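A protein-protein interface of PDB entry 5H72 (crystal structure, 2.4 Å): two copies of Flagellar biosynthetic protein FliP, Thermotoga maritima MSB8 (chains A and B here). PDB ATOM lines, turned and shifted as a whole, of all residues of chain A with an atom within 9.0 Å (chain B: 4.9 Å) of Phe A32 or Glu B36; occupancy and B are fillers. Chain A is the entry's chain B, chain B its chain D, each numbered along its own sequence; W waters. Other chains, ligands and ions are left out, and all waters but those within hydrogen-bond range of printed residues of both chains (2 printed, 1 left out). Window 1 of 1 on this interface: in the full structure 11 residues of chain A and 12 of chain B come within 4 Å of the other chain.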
ATOM      1  N   ARG A  24      10.534  15.671  -1.445  1.00  0.00           N
ATOM      2  CA  ARG A  24      10.634  14.358  -0.832  1.00  0.00           C
ATOM      3  C   ARG A  24       9.932  13.294  -1.683  1.00  0.00           C
ATOM      4  O   ARG A  24      10.412  12.162  -1.785  1.00  0.00           O
ATOM      5  CB  ARG A  24      10.066  14.390   0.591  1.00  0.00           C
ATOM      6  CG  ARG A  24      10.759  15.439   1.462  1.00  0.00           C
ATOM      7  CD  ARG A  24      10.495  15.258   2.944  1.00  0.00           C
ATOM      8  NE  ARG A  24      11.224  14.115   3.480  1.00  0.00           N
ATOM      9  CZ  ARG A  24      11.112  13.674   4.729  1.00  0.00           C
ATOM     10  NH1 ARG A  24      10.296  14.291   5.576  1.00  0.00           N
ATOM     11  NH2 ARG A  24      11.810  12.613   5.126  1.00  0.00           N
ATOM     12  N   VAL A  25       8.808  13.659  -2.299  1.00  0.00           N
ATOM     13  CA  VAL A  25       8.125  12.758  -3.218  1.00  0.00           C
ATOM     14  C   VAL A  25       9.055  12.447  -4.382  1.00  0.00           C
ATOM     15  O   VAL A  25       9.260  11.286  -4.735  1.00  0.00           O
ATOM     16  CB  VAL A  25       6.800  13.352  -3.745  1.00  0.00           C
ATOM     17  CG1 VAL A  25       6.176  12.429  -4.801  1.00  0.00           C
ATOM     18  CG2 VAL A  25       5.826  13.589  -2.602  1.00  0.00           C
ATOM     19  N   ASN A  26       9.622  13.500  -4.956  1.00  0.00           N
ATOM     20  CA  ASN A  26      10.569  13.385  -6.057  1.00  0.00           C
ATOM     21  C   ASN A  26      11.734  12.463  -5.710  1.00  0.00           C
ATOM     22  O   ASN A  26      12.132  11.626  -6.513  1.00  0.00           O
ATOM     23  CB  ASN A  26      11.087  14.777  -6.441  1.00  0.00           C
ATOM     24  CG  ASN A  26      12.056  14.753  -7.625  1.00  0.00           C
ATOM     25  OD1 ASN A  26      11.657  14.553  -8.771  1.00  0.00           O
ATOM     26  ND2 ASN A  26      13.331  14.995  -7.348  1.00  0.00           N
ATOM     27  N   THR A  27      12.274  12.615  -4.505  1.00  0.00           N
ATOM     28  CA  THR A  27      13.413  11.815  -4.083  1.00  0.00           C
ATOM     29  C   THR A  27      13.042  10.346  -3.948  1.00  0.00           C
ATOM     30  O   THR A  27      13.770   9.470  -4.416  1.00  0.00           O
ATOM     31  CB  THR A  27      13.983  12.310  -2.752  1.00  0.00           C
ATOM     32  OG1 THR A  27      14.477  13.637  -2.924  1.00  0.00           O
ATOM     33  CG2 THR A  27      15.128  11.416  -2.295  1.00  0.00           C
ATOM     34  N   ARG A  28      11.912  10.088  -3.300  1.00  0.00           N
ATOM     35  CA  ARG A  28      11.390   8.740  -3.181  1.00  0.00           C
ATOM     36  C   ARG A  28      11.201   8.067  -4.547  1.00  0.00           C
ATOM     37  O   ARG A  28      11.557   6.902  -4.738  1.00  0.00           O
ATOM     38  CB  ARG A  28      10.068   8.756  -2.424  1.00  0.00           C
ATOM     39  CG  ARG A  28       9.371   7.407  -2.375  1.00  0.00           C
ATOM     40  CD  ARG A  28       9.887   6.526  -1.236  1.00  0.00           C
ATOM     41  NE  ARG A  28      11.305   6.180  -1.336  1.00  0.00           N
ATOM     42  CZ  ARG A  28      11.771   5.038  -1.837  1.00  0.00           C
ATOM     43  NH1 ARG A  28      10.928   4.127  -2.313  1.00  0.00           N
ATOM     44  NH2 ARG A  28      13.083   4.808  -1.865  1.00  0.00           N
ATOM     45  N   ILE A  29      10.666   8.808  -5.504  1.00  0.00           N
ATOM     46  CA  ILE A  29      10.382   8.255  -6.822  1.00  0.00           C
ATOM     47  C   ILE A  29      11.667   7.974  -7.599  1.00  0.00           C
ATOM     48  O   ILE A  29      11.789   6.929  -8.246  1.00  0.00           O
ATOM     49  CB  ILE A  29       9.478   9.195  -7.630  1.00  0.00           C
ATOM     50  CG1 ILE A  29       8.079   9.219  -7.021  1.00  0.00           C
ATOM     51  CG2 ILE A  29       9.374   8.740  -9.071  1.00  0.00           C
ATOM     52  CD1 ILE A  29       7.109  10.124  -7.782  1.00  0.00           C
ATOM     53  N   ARG A  30      12.623   8.900  -7.534  1.00  0.00           N
ATOM     54  CA  ARG A  30      13.927   8.675  -8.148  1.00  0.00           C
ATOM     55  C   ARG A  30      14.613   7.449  -7.549  1.00  0.00           C
ATOM     56  O   ARG A  30      15.250   6.676  -8.267  1.00  0.00           O
ATOM     57  CB  ARG A  30      14.833   9.900  -7.979  1.00  0.00           C
ATOM     58  CG  ARG A  30      14.438  11.121  -8.807  1.00  0.00           C
ATOM     59  CD  ARG A  30      15.453  12.240  -8.638  1.00  0.00           C
ATOM     60  NE  ARG A  30      16.811  11.784  -8.924  1.00  0.00           N
ATOM     61  CZ  ARG A  30      17.382  11.830 -10.125  1.00  0.00           C
ATOM     62  NH1 ARG A  30      16.723  12.316 -11.168  1.00  0.00           N
ATOM     63  NH2 ARG A  30      18.620  11.387 -10.284  1.00  0.00           N
ATOM     64  N   GLU A  31      14.485   7.276  -6.235  1.00  0.00           N
ATOM     65  CA  GLU A  31      15.128   6.162  -5.560  1.00  0.00           C
ATOM     66  C   GLU A  31      14.546   4.821  -5.983  1.00  0.00           C
ATOM     67  O   GLU A  31      15.298   3.893  -6.250  1.00  0.00           O
ATOM     68  CB  GLU A  31      15.035   6.318  -4.043  1.00  0.00           C
ATOM     69  CG  GLU A  31      15.998   7.357  -3.496  1.00  0.00           C
ATOM     70  CD  GLU A  31      15.807   7.617  -2.012  1.00  0.00           C
ATOM     71  OE1 GLU A  31      14.886   7.023  -1.410  1.00  0.00           O
ATOM     72  OE2 GLU A  31      16.581   8.417  -1.451  1.00  0.00           O
ATOM     73  N   PHE A  32      13.223   4.697  -6.076  1.00  0.00           N
ATOM     74  CA  PHE A  32      12.717   3.386  -6.442  1.00  0.00           C
ATOM     75  C   PHE A  32      12.877   3.148  -7.942  1.00  0.00           C
ATOM     76  O   PHE A  32      12.936   2.000  -8.371  1.00  0.00           O
ATOM     77  CB  PHE A  32      11.266   3.141  -5.935  1.00  0.00           C
ATOM     78  CG  PHE A  32      10.155   3.859  -6.675  1.00  0.00           C
ATOM     79  CD1 PHE A  32       9.874   3.605  -8.016  1.00  0.00           C
ATOM     80  CD2 PHE A  32       9.299   4.712  -5.975  1.00  0.00           C
ATOM     81  CE1 PHE A  32       8.824   4.248  -8.670  1.00  0.00           C
ATOM     82  CE2 PHE A  32       8.232   5.363  -6.614  1.00  0.00           C
ATOM     83  CZ  PHE A  32       7.993   5.128  -7.967  1.00  0.00           C
ATOM     84  N   MET A  33      13.011   4.202  -8.741  1.00  0.00           N
ATOM     85  CA  MET A  33      13.306   3.978 -10.164  1.00  0.00           C
ATOM     86  C   MET A  33      14.745   3.490 -10.341  1.00  0.00           C
ATOM     87  O   MET A  33      15.008   2.547 -11.075  1.00  0.00           O
ATOM     88  CB  MET A  33      13.075   5.235 -10.996  1.00  0.00           C
ATOM     89  CG  MET A  33      11.607   5.637 -11.102  1.00  0.00           C
ATOM     90  SD  MET A  33      11.330   6.956 -12.296  1.00  0.00           S
ATOM     91  CE  MET A  33      12.486   8.198 -11.748  1.00  0.00           C
ATOM     92  N   ILE A  34      15.671   4.139  -9.652  1.00  0.00           N
ATOM     93  CA  ILE A  34      17.067   3.745  -9.677  1.00  0.00           C
ATOM     94  C   ILE A  34      17.241   2.312  -9.161  1.00  0.00           C
ATOM     95  O   ILE A  34      17.968   1.511  -9.748  1.00  0.00           O
ATOM     96  CB  ILE A  34      17.909   4.737  -8.853  1.00  0.00           C
ATOM     97  CG1 ILE A  34      18.169   5.997  -9.683  1.00  0.00           C
ATOM     98  CG2 ILE A  34      19.216   4.099  -8.386  1.00  0.00           C
ATOM     99  CD1 ILE A  34      18.442   7.215  -8.859  1.00  0.00           C
ATOM    100  N   ASN A  35      16.528   1.981  -8.095  1.00  0.00           N
ATOM    101  CA  ASN A  35      16.541   0.627  -7.551  1.00  0.00           C
ATOM    102  C   ASN A  35      16.013  -0.416  -8.552  1.00  0.00           C
ATOM    103  O   ASN A  35      16.578  -1.505  -8.662  1.00  0.00           O
ATOM    104  CB  ASN A  35      15.725   0.590  -6.251  1.00  0.00           C
ATOM    105  CG  ASN A  35      15.869  -0.716  -5.498  1.00  0.00           C
ATOM    106  OD1 ASN A  35      14.935  -1.519  -5.440  1.00  0.00           O
ATOM    107  ND2 ASN A  35      17.039  -0.930  -4.900  1.00  0.00           N
ATOM    108  N   GLU A  36      14.944  -0.077  -9.283  1.00  0.00           N
ATOM    109  CA  GLU A  36      14.402  -0.971 -10.301  1.00  0.00           C
ATOM    110  C   GLU A  36      15.373  -1.168 -11.450  1.00  0.00           C
ATOM    111  O   GLU A  36      15.532  -2.275 -11.955  1.00  0.00           O
ATOM    112  CB  GLU A  36      13.073  -0.453 -10.852  1.00  0.00           C
ATOM    113  CG  GLU A  36      11.871  -0.722  -9.962  1.00  0.00           C
ATOM    114  CD  GLU A  36      11.439  -2.186  -9.949  1.00  0.00           C
ATOM    115  OE1 GLU A  36      11.154  -2.748 -11.024  1.00  0.00           O
ATOM    116  OE2 GLU A  36      11.368  -2.775  -8.851  1.00  0.00           O
ATOM    117  N   LEU A  37      16.022  -0.093 -11.871  1.00  0.00           N
ATOM    118  CA  LEU A  37      16.957  -0.174 -12.989  1.00  0.00           C
ATOM    119  C   LEU A  37      18.173  -1.039 -12.644  1.00  0.00           C
ATOM    120  O   LEU A  37      18.708  -1.747 -13.494  1.00  0.00           O
ATOM    121  CB  LEU A  37      17.399   1.225 -13.412  1.00  0.00           C
ATOM    122  CG  LEU A  37      16.333   2.056 -14.138  1.00  0.00           C
ATOM    123  CD1 LEU A  37      16.699   3.528 -14.136  1.00  0.00           C
ATOM    124  CD2 LEU A  37      16.145   1.562 -15.554  1.00  0.00           C
ATOM    125  N   LYS A  38      18.600  -0.983 -11.388  1.00  0.00           N
ATOM    126  CA  LYS A  38      19.759  -1.749 -10.949  1.00  0.00           C
ATOM    127  C   LYS A  38      19.410  -3.216 -10.747  1.00  0.00           C
ATOM    128  O   LYS A  38      20.127  -4.096 -11.204  1.00  0.00           O
ATOM    129  CB  LYS A  38      20.334  -1.167  -9.656  1.00  0.00           C
ATOM    130  CG  LYS A  38      21.043   0.161  -9.849  1.00  0.00           C
ATOM    131  CD  LYS A  38      21.543   0.722  -8.519  1.00  0.00           C
ATOM    132  CE  LYS A  38      22.544   1.854  -8.747  1.00  0.00           C
ATOM    133  NZ  LYS A  38      22.929   2.546  -7.482  1.00  0.00           N
ATOM    134  N   ASN A  39      18.302  -3.472 -10.059  1.00  0.00           N
ATOM    135  CA  ASN A  39      17.879  -4.834  -9.770  1.00  0.00           C
ATOM    136  C   ASN A  39      17.581  -5.654 -11.026  1.00  0.00           C
ATOM    137  O   ASN A  39      17.604  -6.882 -10.981  1.00  0.00           O
ATOM    138  CB  ASN A  39      16.647  -4.828  -8.859  1.00  0.00           C
ATOM    139  CG  ASN A  39      16.954  -4.307  -7.462  1.00  0.00           C
ATOM    140  OD1 ASN A  39      18.115  -4.207  -7.065  1.00  0.00           O
ATOM    141  ND2 ASN A  39      15.911  -3.978  -6.708  1.00  0.00           N
ATOM    142  N   HIS A  40      17.295  -4.983 -12.137  1.00  0.00           N
ATOM    143  CA  HIS A  40      17.025  -5.672 -13.396  1.00  0.00           C
ATOM    144  C   HIS A  40      18.108  -5.354 -14.416  1.00  0.00           C
ATOM    145  O   HIS A  40      17.953  -5.619 -15.606  1.00  0.00           O
ATOM    146  CB  HIS A  40      15.635  -5.303 -13.936  1.00  0.00           C
ATOM    147  CG  HIS A  40      14.522  -5.661 -13.006  1.00  0.00           C
ATOM    148  ND1 HIS A  40      14.081  -6.958 -12.837  1.00  0.00           N
ATOM    149  CD2 HIS A  40      13.778  -4.897 -12.169  1.00  0.00           C
ATOM    150  CE1 HIS A  40      13.107  -6.975 -11.942  1.00  0.00           C
ATOM    151  NE2 HIS A  40      12.904  -5.738 -11.525  1.00  0.00           N
ATOM    152  N   ILE A  60      24.024   6.565 -12.617  1.00  0.00           N
ATOM    153  CA  ILE A  60      22.665   6.808 -13.073  1.00  0.00           C
ATOM    154  C   ILE A  60      21.980   7.738 -12.083  1.00  0.00           C
ATOM    155  O   ILE A  60      21.009   8.417 -12.423  1.00  0.00           O
ATOM    156  CB  ILE A  60      21.851   5.510 -13.238  1.00  0.00           C
ATOM    157  CG1 ILE A  60      21.756   4.750 -11.918  1.00  0.00           C
ATOM    158  CG2 ILE A  60      22.455   4.640 -14.323  1.00  0.00           C
ATOM    159  CD1 ILE A  60      20.748   3.629 -11.954  1.00  0.00           C
ATOM    160  N   LEU A  68      16.018   9.709 -16.666  1.00  0.00           N
ATOM    161  CA  LEU A  68      15.772   8.651 -15.697  1.00  0.00           C
ATOM    162  C   LEU A  68      14.383   8.051 -15.878  1.00  0.00           C
ATOM    163  O   LEU A  68      14.227   6.824 -15.868  1.00  0.00           O
ATOM    164  CB  LEU A  68      15.931   9.187 -14.275  1.00  0.00           C
ATOM    165  CG  LEU A  68      15.884   8.162 -13.148  1.00  0.00           C
ATOM    166  CD1 LEU A  68      16.906   7.077 -13.413  1.00  0.00           C
ATOM    167  CD2 LEU A  68      16.142   8.843 -11.810  1.00  0.00           C
ATOM    168  N   ILE A  69      13.375   8.904 -16.058  1.00  0.00           N
ATOM    169  CA  ILE A  69      11.999   8.413 -16.091  1.00  0.00           C
ATOM    170  C   ILE A  69      11.726   7.558 -17.338  1.00  0.00           C
ATOM    171  O   ILE A  69      11.221   6.446 -17.207  1.00  0.00           O
ATOM    172  CB  ILE A  69      10.968   9.567 -15.993  1.00  0.00           C
ATOM    173  CG1 ILE A  69      11.001  10.189 -14.597  1.00  0.00           C
ATOM    174  CG2 ILE A  69       9.567   9.065 -16.297  1.00  0.00           C
ATOM    175  CD1 ILE A  69      10.071  11.383 -14.444  1.00  0.00           C
ATOM    176  N   PHE A  72      13.513   4.229 -16.970  1.00  0.00           N
ATOM    177  CA  PHE A  72      12.794   3.361 -16.044  1.00  0.00           C
ATOM    178  C   PHE A  72      11.616   2.676 -16.738  1.00  0.00           C
ATOM    179  O   PHE A  72      11.402   1.469 -16.576  1.00  0.00           O
ATOM    180  CB  PHE A  72      12.326   4.164 -14.816  1.00  0.00           C
ATOM    181  CG  PHE A  72      11.215   3.508 -14.024  1.00  0.00           C
ATOM    182  CD1 PHE A  72      11.486   2.473 -13.144  1.00  0.00           C
ATOM    183  CD2 PHE A  72       9.898   3.949 -14.143  1.00  0.00           C
ATOM    184  CE1 PHE A  72      10.461   1.875 -12.403  1.00  0.00           C
ATOM    185  CE2 PHE A  72       8.869   3.349 -13.406  1.00  0.00           C
ATOM    186  CZ  PHE A  72       9.155   2.312 -12.536  1.00  0.00           C
ATOM    187  N   GLU A  76      10.977  -1.343 -17.276  1.00  0.00           N
ATOM    188  CA  GLU A  76       9.799  -2.108 -16.854  1.00  0.00           C
ATOM    189  C   GLU A  76       9.156  -2.859 -18.018  1.00  0.00           C
ATOM    190  O   GLU A  76       8.746  -4.011 -17.861  1.00  0.00           O
ATOM    191  CB  GLU A  76       8.749  -1.206 -16.195  1.00  0.00           C
ATOM    192  CG  GLU A  76       9.221  -0.524 -14.912  1.00  0.00           C
ATOM    193  CD  GLU A  76       9.714  -1.507 -13.861  1.00  0.00           C
ATOM    194  OE1 GLU A  76       9.107  -2.590 -13.709  1.00  0.00           O
ATOM    195  OE2 GLU A  76      10.721  -1.197 -13.185  1.00  0.00           O
ATOM    196  N   PHE B  32       6.577  -5.097  -8.651  1.00  0.00           N
ATOM    197  CA  PHE B  32       7.431  -4.089  -8.023  1.00  0.00           C
ATOM    198  C   PHE B  32       6.732  -3.402  -6.835  1.00  0.00           C
ATOM    199  O   PHE B  32       7.399  -2.919  -5.934  1.00  0.00           O
ATOM    200  CB  PHE B  32       7.996  -3.075  -9.053  1.00  0.00           C
ATOM    201  CG  PHE B  32       7.023  -2.059  -9.594  1.00  0.00           C
ATOM    202  CD1 PHE B  32       6.423  -1.102  -8.772  1.00  0.00           C
ATOM    203  CD2 PHE B  32       6.812  -1.981 -10.968  1.00  0.00           C
ATOM    204  CE1 PHE B  32       5.570  -0.166  -9.282  1.00  0.00           C
ATOM    205  CE2 PHE B  32       5.954  -1.017 -11.506  1.00  0.00           C
ATOM    206  CZ  PHE B  32       5.329  -0.113 -10.658  1.00  0.00           C
ATOM    207  N   MET B  33       5.402  -3.400  -6.808  1.00  0.00           N
ATOM    208  CA  MET B  33       4.694  -2.926  -5.619  1.00  0.00           C
ATOM    209  C   MET B  33       4.964  -3.842  -4.434  1.00  0.00           C
ATOM    210  O   MET B  33       5.290  -3.384  -3.345  1.00  0.00           O
ATOM    211  CB  MET B  33       3.201  -2.832  -5.875  1.00  0.00           C
ATOM    212  CG  MET B  33       2.846  -1.702  -6.824  1.00  0.00           C
ATOM    213  SD  MET B  33       1.083  -1.363  -6.827  1.00  0.00           S
ATOM    214  CE  MET B  33       0.423  -2.940  -7.368  1.00  0.00           C
ATOM    215  N   ILE B  34       4.845  -5.143  -4.670  1.00  0.00           N
ATOM    216  CA  ILE B  34       5.091  -6.136  -3.638  1.00  0.00           C
ATOM    217  C   ILE B  34       6.545  -6.080  -3.168  1.00  0.00           C
ATOM    218  O   ILE B  34       6.829  -6.102  -1.964  1.00  0.00           O
ATOM    219  CB  ILE B  34       4.741  -7.544  -4.152  1.00  0.00           C
ATOM    220  CG1 ILE B  34       3.222  -7.725  -4.153  1.00  0.00           C
ATOM    221  CG2 ILE B  34       5.418  -8.617  -3.320  1.00  0.00           C
ATOM    222  CD1 ILE B  34       2.723  -8.659  -5.239  1.00  0.00           C
ATOM    223  N   ASN B  35       7.457  -5.980  -4.127  1.00  0.00           N
ATOM    224  CA  ASN B  35       8.874  -5.842  -3.823  1.00  0.00           C
ATOM    225  C   ASN B  35       9.146  -4.612  -2.951  1.00  0.00           C
ATOM    226  O   ASN B  35       9.851  -4.707  -1.951  1.00  0.00           O
ATOM    227  CB  ASN B  35       9.671  -5.775  -5.120  1.00  0.00           C
ATOM    228  CG  ASN B  35      11.162  -5.802  -4.898  1.00  0.00           C
ATOM    229  OD1 ASN B  35      11.838  -4.786  -5.034  1.00  0.00           O
ATOM    230  ND2 ASN B  35      11.694  -6.975  -4.581  1.00  0.00           N
ATOM    231  N   GLU B  36       8.566  -3.466  -3.319  1.00  0.00           N
ATOM    232  CA  GLU B  36       8.727  -2.233  -2.548  1.00  0.00           C
ATOM    233  C   GLU B  36       8.165  -2.369  -1.137  1.00  0.00           C
ATOM    234  O   GLU B  36       8.732  -1.832  -0.185  1.00  0.00           O
ATOM    235  CB  GLU B  36       8.050  -1.046  -3.250  1.00  0.00           C
ATOM    236  CG  GLU B  36       8.870  -0.406  -4.356  1.00  0.00           C
ATOM    237  CD  GLU B  36      10.041   0.409  -3.823  1.00  0.00           C
ATOM    238  OE1 GLU B  36       9.808   1.421  -3.119  1.00  0.00           O
ATOM    239  OE2 GLU B  36      11.196   0.044  -4.115  1.00  0.00           O
ATOM    240  N   LEU B  37       7.048  -3.085  -1.011  1.00  0.00           N
ATOM    241  CA  LEU B  37       6.404  -3.261   0.278  1.00  0.00           C
ATOM    242  C   LEU B  37       7.236  -4.128   1.241  1.00  0.00           C
ATOM    243  O   LEU B  37       7.279  -3.852   2.442  1.00  0.00           O
ATOM    244  CB  LEU B  37       5.009  -3.851   0.091  1.00  0.00           C
ATOM    245  CG  LEU B  37       3.966  -2.867  -0.455  1.00  0.00           C
ATOM    246  CD1 LEU B  37       2.754  -3.606  -0.967  1.00  0.00           C
ATOM    247  CD2 LEU B  37       3.561  -1.842   0.595  1.00  0.00           C
ATOM    248  N   LYS B  38       7.889  -5.166   0.714  1.00  0.00           N
ATOM    249  CA  LYS B  38       8.720  -6.042   1.539  1.00  0.00           C
ATOM    250  C   LYS B  38       9.997  -5.336   1.922  1.00  0.00           C
ATOM    251  O   LYS B  38      10.378  -5.328   3.087  1.00  0.00           O
ATOM    252  CB  LYS B  38       9.052  -7.350   0.817  1.00  0.00           C
ATOM    253  CG  LYS B  38       7.833  -8.236   0.588  1.00  0.00           C
ATOM    254  CD  LYS B  38       8.200  -9.595   0.014  1.00  0.00           C
ATOM    255  CE  LYS B  38       6.923 -10.415  -0.228  1.00  0.00           C
ATOM    256  NZ  LYS B  38       7.136 -11.679  -1.010  1.00  0.00           N
ATOM    257  N   ASN B  39      10.643  -4.725   0.936  1.00  0.00           N
ATOM    258  CA  ASN B  39      11.947  -4.107   1.138  1.00  0.00           C
ATOM    259  C   ASN B  39      11.935  -2.944   2.139  1.00  0.00           C
ATOM    260  O   ASN B  39      12.958  -2.617   2.729  1.00  0.00           O
ATOM    261  CB  ASN B  39      12.509  -3.651  -0.208  1.00  0.00           C
ATOM    262  CG  ASN B  39      13.037  -4.822  -1.034  1.00  0.00           C
ATOM    263  OD1 ASN B  39      13.001  -5.969  -0.587  1.00  0.00           O
ATOM    264  ND2 ASN B  39      13.521  -4.537  -2.239  1.00  0.00           N
ATOM    265  N   HIS B  40      10.770  -2.343   2.343  1.00  0.00           N
ATOM    266  CA  HIS B  40      10.626  -1.298   3.344  1.00  0.00           C
ATOM    267  C   HIS B  40       9.730  -1.773   4.489  1.00  0.00           C
ATOM    268  O   HIS B  40       9.267  -0.978   5.299  1.00  0.00           O
ATOM    269  CB  HIS B  40      10.058  -0.024   2.717  1.00  0.00           C
ATOM    270  CG  HIS B  40      10.912   0.543   1.627  1.00  0.00           C
ATOM    271  ND1 HIS B  40      12.117   1.165   1.870  1.00  0.00           N
ATOM    272  CD2 HIS B  40      10.735   0.577   0.287  1.00  0.00           C
ATOM    273  CE1 HIS B  40      12.646   1.563   0.726  1.00  0.00           C
ATOM    274  NE2 HIS B  40      11.826   1.213  -0.253  1.00  0.00           N
ATOM    275  N   PHE B  72       0.531   0.161  -1.245  1.00  0.00           N
ATOM    276  CA  PHE B  72       1.814   0.510  -1.849  1.00  0.00           C
ATOM    277  C   PHE B  72       2.014   2.007  -1.773  1.00  0.00           C
ATOM    278  O   PHE B  72       3.116   2.471  -1.509  1.00  0.00           O
ATOM    279  CB  PHE B  72       1.880   0.011  -3.307  1.00  0.00           C
ATOM    280  CG  PHE B  72       2.920   0.701  -4.156  1.00  0.00           C
ATOM    281  CD1 PHE B  72       4.257   0.349  -4.065  1.00  0.00           C
ATOM    282  CD2 PHE B  72       2.554   1.708  -5.051  1.00  0.00           C
ATOM    283  CE1 PHE B  72       5.221   0.983  -4.845  1.00  0.00           C
ATOM    284  CE2 PHE B  72       3.508   2.349  -5.834  1.00  0.00           C
ATOM    285  CZ  PHE B  72       4.843   1.986  -5.737  1.00  0.00           C
ATOM    286  N   GLU B  76       4.900   4.121   0.213  1.00  0.00           N
ATOM    287  CA  GLU B  76       5.871   5.026  -0.404  1.00  0.00           C
ATOM    288  C   GLU B  76       5.872   6.399   0.255  1.00  0.00           C
ATOM    289  O   GLU B  76       6.906   7.027   0.359  1.00  0.00           O
ATOM    290  CB  GLU B  76       5.601   5.186  -1.896  1.00  0.00           C
ATOM    291  CG  GLU B  76       5.758   3.915  -2.708  1.00  0.00           C
ATOM    292  CD  GLU B  76       7.167   3.404  -2.728  1.00  0.00           C
ATOM    293  OE1 GLU B  76       8.105   4.228  -2.780  1.00  0.00           O
ATOM    294  OE2 GLU B  76       7.337   2.171  -2.679  1.00  0.00           O
HETATM  295  O   HOH W   1      15.949  -4.359  -3.841  1.00  0.00           O
HETATM  296  O   HOH W   2      12.864   1.964  -2.880  1.00  0.00           O
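Among the printed residues, merely in contact across the chains: Glu A36 with Phe B32, Phe A32 with Glu B76, Phe A32 with Glu B36, Glu A76 with Phe B32 and Arg A28 with His B40.
The guanidinium group of Arg A28 lies within salt-bridge range of the side-chain carboxylate of Glu B36. The guanidinium group (NH1) of Arg A28 is in salt-bridge range of the side-chain carboxylate (OE1) of Glu B76 (2.9 Å).
Phe A32 touches Glu B36, and with the chains exchanged Glu A36 touches Phe B32. Phe A32 touches Glu B76, and with the chains exchanged Glu A76 touches Phe B32. Of the 7 pairs that touch across the chains among the printed residues, 4 have their exchanged pair printed and touching as well.
Of chain B, only Glu B36 (3.6 Å) and Glu B76 (3.4 Å) come within 4 Å of Phe A32. Printed residues of chain B within 4 Å of Glu A36: Phe B32 (3.4 Å). Of the printed residues of chain B, Glu A76 touches Phe B32. Printed residues of chain A within 4 Å of Phe B32: Glu A36 (3.4 Å) and Glu A76 (3.6 Å). No residue of chain A comes within 4 Å of Asn B35. Of the printed residues of chain A, His B40 touches Arg A28. Printed residues of chain A within 4 Å of Glu B76: Arg A28 (2.9 Å) and Phe A32 (3.4 Å). The nearest printed residue of chain B that does not touch Phe A32 is Phe B72 (4.9 Å). The nearest residue of chain A that does not touch Glu B36 is Asn A35 (4.3 Å). The nearest printed residue of chain B that does not touch Arg A28 is Phe B72 (7.0 Å).
Printed residues of chain A that touch a printed residue of chain B: Arg A28, Phe A32, Glu A36 and Glu A76. Hydrophobic or aromatic side chains of chain A within 4 Å of the printed part of chain B: Phe A32.
Water W2 lies within hydrogen-bond range of OE2 of Glu B36 (2.8 Å), NE2 of His B40 (2.9 Å) and NH1 of Arg A28 (3.0 Å). Water W1 lies within hydrogen-bond range of the side-chain amide nitrogen of Asn A39 (2.9 Å), the side-chain amide nitrogen of Asn B39 (2.9 Å) and the side-chain amide oxygen of Asn A35 (3.4 Å).
The guanidinium group (NH2) of Arg A28 lies within salt-bridge range of the side-chain carboxylate (OE1) of Glu A31. The side-chain carboxylate of Glu A76 lies close to the side-chain carboxylate of Glu A36. The side-chain carboxylate (OE1) of Glu B36 sits close to the side-chain carboxylate (OE2) of Glu B76, 2.6 Å away.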
